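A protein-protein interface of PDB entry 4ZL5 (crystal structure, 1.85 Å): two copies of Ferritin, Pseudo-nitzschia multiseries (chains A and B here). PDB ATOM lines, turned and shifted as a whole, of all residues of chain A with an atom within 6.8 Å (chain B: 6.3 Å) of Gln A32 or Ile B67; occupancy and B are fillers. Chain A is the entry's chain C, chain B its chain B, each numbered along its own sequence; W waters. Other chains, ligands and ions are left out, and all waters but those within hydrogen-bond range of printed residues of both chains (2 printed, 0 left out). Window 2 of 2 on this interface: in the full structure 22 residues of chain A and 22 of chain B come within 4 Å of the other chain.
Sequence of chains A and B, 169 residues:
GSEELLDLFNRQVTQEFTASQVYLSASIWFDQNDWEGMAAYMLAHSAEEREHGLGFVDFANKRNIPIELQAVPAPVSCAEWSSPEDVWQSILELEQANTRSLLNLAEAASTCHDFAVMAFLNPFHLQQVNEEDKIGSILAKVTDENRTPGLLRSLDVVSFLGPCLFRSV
CD1 of Leu B69 touches N of Ser A25, 3.9 Å away.
CG1 of Ile A28 touches CG1 of Val B57, at 3.6 Å.
Asn B61 touches Ile A28.
Ile B67 touches Ile A28 (CG2 to CD1, 3.9 Å).
Ile A28 touches Leu B69 (CD1 to CG, 3.99 Å).
Asp A31 touches Asn B61.
Gln A32 touches Ile B67.
The side-chain hydroxyl (OG) of Ser A25 lies within hydrogen-bond range of SG of YCM A78, at 3.5 Å.
O of Val B57 lies close to OD1 of Asn B61 (3.5 Å).
Of the 12 printed residues of chain A, 4 touch a printed residue of chain B.
Hydrophobic or aromatic side chains of chain A that line the printed part of chain B: Ile A28.
Along chain A the printed residues that touch a printed residue of chain B span positions 25 to 32.
Printed residues of chain B within 4 Å of Ser A25: Leu B69 (3.9 Å).
Of the printed residues of chain B, Asp A31 touches Asn B61.
Gln A32 touches just one residue of chain B: Ile B67 (3.9 Å).
Of the printed residues of chain A, Val B57 touches Ile A28.
Of the printed residues of chain A, Asn B61 touches Ile A28 (3.9 Å) and Asp A31 (3.7 Å).
Of the printed residues of chain A, Ile B67 touches Ile A28 and Gln A32.
Printed residues of chain A within 4 Å of Leu B69: Ser A25 (3.9 Å) and Ile A28 (3.99 Å).
The nearest printed residue of chain B that does not touch Gln A32 is Pro B66 (4.1 Å).
The nearest printed residue of chain A that does not touch Ile B67 is YCM A78 (6.6 Å).
Water W1 lies within hydrogen-bond range of the side-chain amide oxygen of Asn B61 (2.5 Å), the side-chain amide nitrogen of Gln A32 (2.8 Å), the backbone carbonyl oxygen of Ile B65 (2.9 Å) and the backbone NH of Ile B67 (3.4 Å).
Water W2 lies within hydrogen-bond range of OD2 of Asp A31 (2.9 Å), OG of Ser A27 (2.9 Å) and ND2 of Asn B61 (2.9 Å).
No position is printed for both chains.
Of the 7 pairs that touch across the chains among the printed residues, none has its exchanged pair printed and touching as well.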
ATOM      1  N   SER A  25      24.040  17.942  27.368  1.00  0.00           N
ATOM      2  CA  SER A  25      23.114  18.661  28.164  1.00  0.00           C
ATOM      3  C   SER A  25      23.817  19.046  29.473  1.00  0.00           C
ATOM      4  O   SER A  25      23.645  20.186  29.956  1.00  0.00           O
ATOM      5  CB  SER A  25      21.909  17.736  28.508  1.00  0.00           C
ATOM      6  OG  SER A  25      20.960  18.450  29.221  1.00  0.00           O
ATOM      7  N   SER A  27      27.032  19.560  29.982  1.00  0.00           N
ATOM      8  CA  SER A  27      27.941  20.648  29.641  1.00  0.00           C
ATOM      9  C   SER A  27      27.243  21.985  29.531  1.00  0.00           C
ATOM     10  O   SER A  27      27.741  23.018  30.033  1.00  0.00           O
ATOM     11  CB  SER A  27      28.721  20.347  28.346  1.00  0.00           C
ATOM     12  OG  SER A  27      28.006  20.792  27.208  1.00  0.00           O
ATOM     13  N   ILE A  28      26.051  22.001  28.948  1.00  0.00           N
ATOM     14  CA  ILE A  28      25.320  23.239  28.862  1.00  0.00           C
ATOM     15  C   ILE A  28      24.917  23.760  30.247  1.00  0.00           C
ATOM     16  O   ILE A  28      25.007  24.964  30.519  1.00  0.00           O
ATOM     17  CB  ILE A  28      24.086  23.040  27.934  1.00  0.00           C
ATOM     18  CG1 ILE A  28      24.534  22.784  26.463  1.00  0.00           C
ATOM     19  CG2 ILE A  28      23.054  24.160  28.067  1.00  0.00           C
ATOM     20  CD1 ILE A  28      23.411  22.355  25.581  1.00  0.00           C
ATOM     21  N   TRP A  29      24.358  22.895  31.082  1.00  0.00           N
ATOM     22  CA  TRP A  29      24.016  23.289  32.415  1.00  0.00           C
ATOM     23  C   TRP A  29      25.219  23.888  33.142  1.00  0.00           C
ATOM     24  O   TRP A  29      25.107  24.901  33.793  1.00  0.00           O
ATOM     25  CB  TRP A  29      23.380  22.107  33.233  1.00  0.00           C
ATOM     26  CG  TRP A  29      22.766  22.592  34.531  1.00  0.00           C
ATOM     27  CD1 TRP A  29      21.476  22.984  34.735  1.00  0.00           C
ATOM     28  CD2 TRP A  29      23.461  22.856  35.736  1.00  0.00           C
ATOM     29  NE1 TRP A  29      21.324  23.401  36.027  1.00  0.00           N
ATOM     30  CE2 TRP A  29      22.531  23.339  36.662  1.00  0.00           C
ATOM     31  CE3 TRP A  29      24.762  22.665  36.138  1.00  0.00           C
ATOM     32  CZ2 TRP A  29      22.875  23.656  37.972  1.00  0.00           C
ATOM     33  CZ3 TRP A  29      25.117  23.010  37.419  1.00  0.00           C
ATOM     34  CH2 TRP A  29      24.170  23.506  38.330  1.00  0.00           C
ATOM     35  N   PHE A  30      26.334  23.190  33.111  1.00  0.00           N
ATOM     36  CA  PHE A  30      27.553  23.688  33.749  1.00  0.00           C
ATOM     37  C   PHE A  30      28.006  25.013  33.191  1.00  0.00           C
ATOM     38  O   PHE A  30      28.321  25.971  33.960  1.00  0.00           O
ATOM     39  CB  PHE A  30      28.638  22.652  33.595  1.00  0.00           C
ATOM     40  CG  PHE A  30      28.522  21.530  34.568  1.00  0.00           C
ATOM     41  CD1 PHE A  30      28.297  21.757  35.951  1.00  0.00           C
ATOM     42  CD2 PHE A  30      28.714  20.273  34.162  1.00  0.00           C
ATOM     43  CE1 PHE A  30      28.208  20.712  36.850  1.00  0.00           C
ATOM     44  CE2 PHE A  30      28.661  19.232  35.053  1.00  0.00           C
ATOM     45  CZ  PHE A  30      28.396  19.429  36.402  1.00  0.00           C
ATOM     46  N   ASP A  31      28.005  25.131  31.876  1.00  0.00           N
ATOM     47  CA  ASP A  31      28.419  26.391  31.263  1.00  0.00           C
ATOM     48  C   ASP A  31      27.482  27.524  31.675  1.00  0.00           C
ATOM     49  O   ASP A  31      27.923  28.592  32.071  1.00  0.00           O
ATOM     50  CB  ASP A  31      28.478  26.332  29.736  1.00  0.00           C
ATOM     51  CG  ASP A  31      29.856  26.065  29.207  1.00  0.00           C
ATOM     52  OD1 ASP A  31      30.823  26.699  29.715  1.00  0.00           O
ATOM     53  OD2 ASP A  31      29.973  25.202  28.275  1.00  0.00           O
ATOM     54  N   GLN A  32      26.189  27.314  31.529  1.00  0.00           N
ATOM     55  CA  GLN A  32      25.220  28.301  31.905  1.00  0.00           C
ATOM     56  C   GLN A  32      25.401  28.753  33.338  1.00  0.00           C
ATOM     57  O   GLN A  32      25.046  29.893  33.635  1.00  0.00           O
ATOM     58  CB  GLN A  32      23.792  27.754  31.717  1.00  0.00           C
ATOM     59  CG  GLN A  32      23.358  27.597  30.267  1.00  0.00           C
ATOM     60  CD  GLN A  32      22.006  26.903  30.128  1.00  0.00           C
ATOM     61  OE1 GLN A  32      21.522  26.181  31.061  1.00  0.00           O
ATOM     62  NE2 GLN A  32      21.379  27.107  28.963  1.00  0.00           N
ATOM     63  N   ASN A  33      25.825  27.844  34.247  1.00  0.00           N
ATOM     64  CA  ASN A  33      25.984  28.190  35.659  1.00  0.00           C
ATOM     65  C   ASN A  33      27.454  28.485  36.068  1.00  0.00           C
ATOM     66  O   ASN A  33      27.778  28.480  37.225  1.00  0.00           O
ATOM     67  CB  ASN A  33      25.343  27.079  36.522  1.00  0.00           C
ATOM     68  CG  ASN A  33      23.828  27.094  36.415  1.00  0.00           C
ATOM     69  OD1 ASN A  33      23.180  27.897  37.052  1.00  0.00           O
ATOM     70  ND2 ASN A  33      23.277  26.262  35.581  1.00  0.00           N
ATOM     71  N   ASP A  34      28.303  28.683  35.075  1.00  0.00           N
ATOM     72  CA  ASP A  34      29.668  29.160  35.228  1.00  0.00           C
ATOM     73  C   ASP A  34      30.596  28.149  35.868  1.00  0.00           C
ATOM     74  O   ASP A  34      31.398  28.533  36.700  1.00  0.00           O
ATOM     75  CB  ASP A  34      29.663  30.458  36.047  1.00  0.00           C
ATOM     76  CG  ASP A  34      28.826  31.515  35.415  1.00  0.00           C
ATOM     77  OD1 ASP A  34      29.065  31.809  34.258  1.00  0.00           O
ATOM     78  OD2 ASP A  34      27.853  31.942  36.045  1.00  0.00           O
ATOM     79  N   TRP A  35      30.417  26.867  35.551  1.00  0.00           N
ATOM     80  CA  TRP A  35      31.277  25.805  36.001  1.00  0.00           C
ATOM     81  C   TRP A  35      32.031  25.336  34.790  1.00  0.00           C
ATOM     82  O   TRP A  35      31.758  24.248  34.244  1.00  0.00           O
ATOM     83  CB  TRP A  35      30.470  24.657  36.581  1.00  0.00           C
ATOM     84  CG  TRP A  35      29.709  24.997  37.767  1.00  0.00           C
ATOM     85  CD1 TRP A  35      28.434  25.383  37.813  1.00  0.00           C
ATOM     86  CD2 TRP A  35      30.166  24.953  39.120  1.00  0.00           C
ATOM     87  NE1 TRP A  35      28.048  25.563  39.100  1.00  0.00           N
ATOM     88  CE2 TRP A  35      29.115  25.347  39.919  1.00  0.00           C
ATOM     89  CE3 TRP A  35      31.374  24.606  39.713  1.00  0.00           C
ATOM     90  CZ2 TRP A  35      29.204  25.411  41.341  1.00  0.00           C
ATOM     91  CZ3 TRP A  35      31.460  24.664  41.118  1.00  0.00           C
ATOM     92  CH2 TRP A  35      30.396  25.070  41.893  1.00  0.00           C
ATOM     93  N   ALA A  39      32.056  21.708  32.729  1.00  0.00           N
ATOM     94  CA  ALA A  39      31.490  21.807  31.426  1.00  0.00           C
ATOM     95  C   ALA A  39      32.434  21.202  30.388  1.00  0.00           C
ATOM     96  O   ALA A  39      31.978  20.413  29.557  1.00  0.00           O
ATOM     97  CB  ALA A  39      31.142  23.219  31.038  1.00  0.00           C
ATOM     98  N   YCM A  78      18.035  17.765  32.764  1.00  0.00           N
ATOM     99  CA  YCM A  78      18.377  19.181  32.912  1.00  0.00           C
ATOM    100  CB  YCM A  78      18.630  19.924  31.590  1.00  0.00           C
ATOM    101  SG  YCM A  78      17.717  19.313  30.145  1.00  0.00           S
ATOM    102  C   YCM A  78      17.291  19.893  33.631  1.00  0.00           C
ATOM    103  O   YCM A  78      17.581  20.659  34.573  1.00  0.00           O
ATOM    104  N   LEU B   6      15.264  33.258  19.443  1.00  0.00           N
ATOM    105  CA  LEU B   6      15.606  32.179  20.327  1.00  0.00           C
ATOM    106  C   LEU B   6      15.195  30.782  19.772  1.00  0.00           C
ATOM    107  O   LEU B   6      15.958  29.784  19.837  1.00  0.00           O
ATOM    108  CB  LEU B   6      14.957  32.437  21.692  1.00  0.00           C
ATOM    109  CG  LEU B   6      14.715  31.196  22.572  1.00  0.00           C
ATOM    110  CD1 LEU B   6      16.045  30.595  22.998  1.00  0.00           C
ATOM    111  CD2 LEU B   6      13.837  31.450  23.812  1.00  0.00           C
ATOM    112  N   PHE B   9      17.306  29.912  16.741  1.00  0.00           N
ATOM    113  CA  PHE B   9      18.636  29.522  17.138  1.00  0.00           C
ATOM    114  C   PHE B   9      18.630  28.090  17.673  1.00  0.00           C
ATOM    115  O   PHE B   9      19.446  27.243  17.278  1.00  0.00           O
ATOM    116  CB  PHE B   9      19.163  30.534  18.178  1.00  0.00           C
ATOM    117  CG  PHE B   9      20.644  30.665  18.190  1.00  0.00           C
ATOM    118  CD1 PHE B   9      21.400  29.687  18.735  1.00  0.00           C
ATOM    119  CD2 PHE B   9      21.267  31.732  17.565  1.00  0.00           C
ATOM    120  CE1 PHE B   9      22.772  29.755  18.698  1.00  0.00           C
ATOM    121  CE2 PHE B   9      22.632  31.809  17.507  1.00  0.00           C
ATOM    122  CZ  PHE B   9      23.390  30.812  18.089  1.00  0.00           C
ATOM    123  N   ASN B  10      17.677  27.754  18.537  1.00  0.00           N
ATOM    124  CA  ASN B  10      17.540  26.400  18.958  1.00  0.00           C
ATOM    125  C   ASN B  10      17.265  25.436  17.870  1.00  0.00           C
ATOM    126  O   ASN B  10      17.772  24.281  17.921  1.00  0.00           O
ATOM    127  CB  ASN B  10      16.387  26.178  19.946  1.00  0.00           C
ATOM    128  CG  ASN B  10      16.831  26.321  21.381  1.00  0.00           C
ATOM    129  OD1 ASN B  10      17.254  25.338  22.068  1.00  0.00           O
ATOM    130  ND2 ASN B  10      16.818  27.576  21.835  1.00  0.00           N
ATOM    131  N   VAL B  13      20.482  24.313  15.997  1.00  0.00           N
ATOM    132  CA  VAL B  13      21.208  23.260  16.706  1.00  0.00           C
ATOM    133  C   VAL B  13      20.652  21.904  16.305  1.00  0.00           C
ATOM    134  O   VAL B  13      21.393  20.994  15.946  1.00  0.00           O
ATOM    135  CB  VAL B  13      21.148  23.446  18.219  1.00  0.00           C
ATOM    136  CG1 VAL B  13      21.827  22.282  18.919  1.00  0.00           C
ATOM    137  CG2 VAL B  13      21.842  24.752  18.547  1.00  0.00           C
ATOM    138  N   PHE B  56      27.253  26.464  17.636  1.00  0.00           N
ATOM    139  CA  PHE B  56      26.034  27.145  17.985  1.00  0.00           C
ATOM    140  C   PHE B  56      25.701  27.104  19.435  1.00  0.00           C
ATOM    141  O   PHE B  56      25.368  28.143  19.999  1.00  0.00           O
ATOM    142  CB  PHE B  56      24.846  26.686  17.161  1.00  0.00           C
ATOM    143  CG  PHE B  56      24.806  27.311  15.754  1.00  0.00           C
ATOM    144  CD1 PHE B  56      25.662  26.864  14.759  1.00  0.00           C
ATOM    145  CD2 PHE B  56      23.941  28.345  15.460  1.00  0.00           C
ATOM    146  CE1 PHE B  56      25.696  27.464  13.502  1.00  0.00           C
ATOM    147  CE2 PHE B  56      23.968  28.954  14.196  1.00  0.00           C
ATOM    148  CZ  PHE B  56      24.843  28.505  13.226  1.00  0.00           C
ATOM    149  N   VAL B  57      25.785  25.927  20.033  1.00  0.00           N
ATOM    150  CA  VAL B  57      25.585  25.788  21.468  1.00  0.00           C
ATOM    151  C   VAL B  57      26.500  26.716  22.292  1.00  0.00           C
ATOM    152  O   VAL B  57      26.021  27.506  23.135  1.00  0.00           O
ATOM    153  CB  VAL B  57      25.760  24.326  21.896  1.00  0.00           C
ATOM    154  CG1 VAL B  57      25.822  24.178  23.415  1.00  0.00           C
ATOM    155  CG2 VAL B  57      24.602  23.451  21.327  1.00  0.00           C
ATOM    156  N   ALA B  60      25.496  30.383  21.873  1.00  0.00           N
ATOM    157  CA  ALA B  60      24.301  30.620  22.616  1.00  0.00           C
ATOM    158  C   ALA B  60      24.584  30.731  24.121  1.00  0.00           C
ATOM    159  O   ALA B  60      23.988  31.623  24.766  1.00  0.00           O
ATOM    160  CB  ALA B  60      23.307  29.494  22.359  1.00  0.00           C
ATOM    161  N   ASN B  61      25.398  29.825  24.662  1.00  0.00           N
ATOM    162  CA  ASN B  61      25.754  29.841  26.068  1.00  0.00           C
ATOM    163  C   ASN B  61      26.398  31.214  26.409  1.00  0.00           C
ATOM    164  O   ASN B  61      26.020  31.892  27.402  1.00  0.00           O
ATOM    165  CB  ASN B  61      26.702  28.705  26.425  1.00  0.00           C
ATOM    166  CG  ASN B  61      26.018  27.306  26.403  1.00  0.00           C
ATOM    167  OD1 ASN B  61      24.763  27.174  26.365  1.00  0.00           O
ATOM    168  ND2 ASN B  61      26.856  26.240  26.409  1.00  0.00           N
ATOM    169  N   ILE B  65      21.506  32.806  25.272  1.00  0.00           N
ATOM    170  CA  ILE B  65      20.382  32.315  24.518  1.00  0.00           C
ATOM    171  C   ILE B  65      20.173  30.899  25.114  1.00  0.00           C
ATOM    172  O   ILE B  65      21.037  30.069  24.974  1.00  0.00           O
ATOM    173  CB  ILE B  65      20.729  32.251  23.042  1.00  0.00           C
ATOM    174  CG1 ILE B  65      21.025  33.660  22.523  1.00  0.00           C
ATOM    175  CG2 ILE B  65      19.622  31.563  22.233  1.00  0.00           C
ATOM    176  CD1 ILE B  65      21.671  33.693  21.150  1.00  0.00           C
ATOM    177  N   PRO B  66      19.095  30.661  25.863  1.00  0.00           N
ATOM    178  CA  PRO B  66      18.932  29.346  26.487  1.00  0.00           C
ATOM    179  C   PRO B  66      18.753  28.238  25.419  1.00  0.00           C
ATOM    180  O   PRO B  66      17.967  28.383  24.491  1.00  0.00           O
ATOM    181  CB  PRO B  66      17.625  29.483  27.299  1.00  0.00           C
ATOM    182  CG  PRO B  66      17.149  30.925  27.146  1.00  0.00           C
ATOM    183  CD  PRO B  66      17.917  31.538  26.018  1.00  0.00           C
ATOM    184  N   ILE B  67      19.530  27.195  25.497  1.00  0.00           N
ATOM    185  CA  ILE B  67      19.429  26.078  24.552  1.00  0.00           C
ATOM    186  C   ILE B  67      18.669  24.963  25.255  1.00  0.00           C
ATOM    187  O   ILE B  67      19.021  24.599  26.356  1.00  0.00           O
ATOM    188  CB  ILE B  67      20.831  25.578  24.167  1.00  0.00           C
ATOM    189  CG1 ILE B  67      21.589  26.626  23.295  1.00  0.00           C
ATOM    190  CG2 ILE B  67      20.716  24.230  23.453  1.00  0.00           C
ATOM    191  CD1 ILE B  67      20.856  26.919  22.019  1.00  0.00           C
ATOM    192  N   GLU B  68      17.635  24.432  24.630  1.00  0.00           N
ATOM    193  CA  GLU B  68      17.112  23.182  25.082  1.00  0.00           C
ATOM    194  C   GLU B  68      17.206  22.178  23.946  1.00  0.00           C
ATOM    195  O   GLU B  68      16.692  22.389  22.861  1.00  0.00           O
ATOM    196  CB  GLU B  68      15.690  23.350  25.535  1.00  0.00           C
ATOM    197  CG  GLU B  68      15.715  24.240  26.786  1.00  0.00           C
ATOM    198  CD  GLU B  68      14.391  24.299  27.505  1.00  0.00           C
ATOM    199  OE1 GLU B  68      13.510  23.476  27.157  1.00  0.00           O
ATOM    200  OE2 GLU B  68      14.263  25.162  28.403  1.00  0.00           O
ATOM    201  N   LEU B  69      17.980  21.161  24.208  1.00  0.00           N
ATOM    202  CA  LEU B  69      18.320  20.162  23.189  1.00  0.00           C
ATOM    203  C   LEU B  69      17.056  19.391  22.893  1.00  0.00           C
ATOM    204  O   LEU B  69      16.409  18.900  23.793  1.00  0.00           O
ATOM    205  CB  LEU B  69      19.381  19.242  23.781  1.00  0.00           C
ATOM    206  CG  LEU B  69      20.809  19.819  23.934  1.00  0.00           C
ATOM    207  CD1 LEU B  69      21.774  18.727  24.342  1.00  0.00           C
ATOM    208  CD2 LEU B  69      21.335  20.394  22.623  1.00  0.00           C
HETATM  209  O   HOH W   1      22.541  28.372  26.701  1.00  0.00           O
HETATM  210  O   HOH W   2      28.224  23.635  26.541  1.00  0.00           O
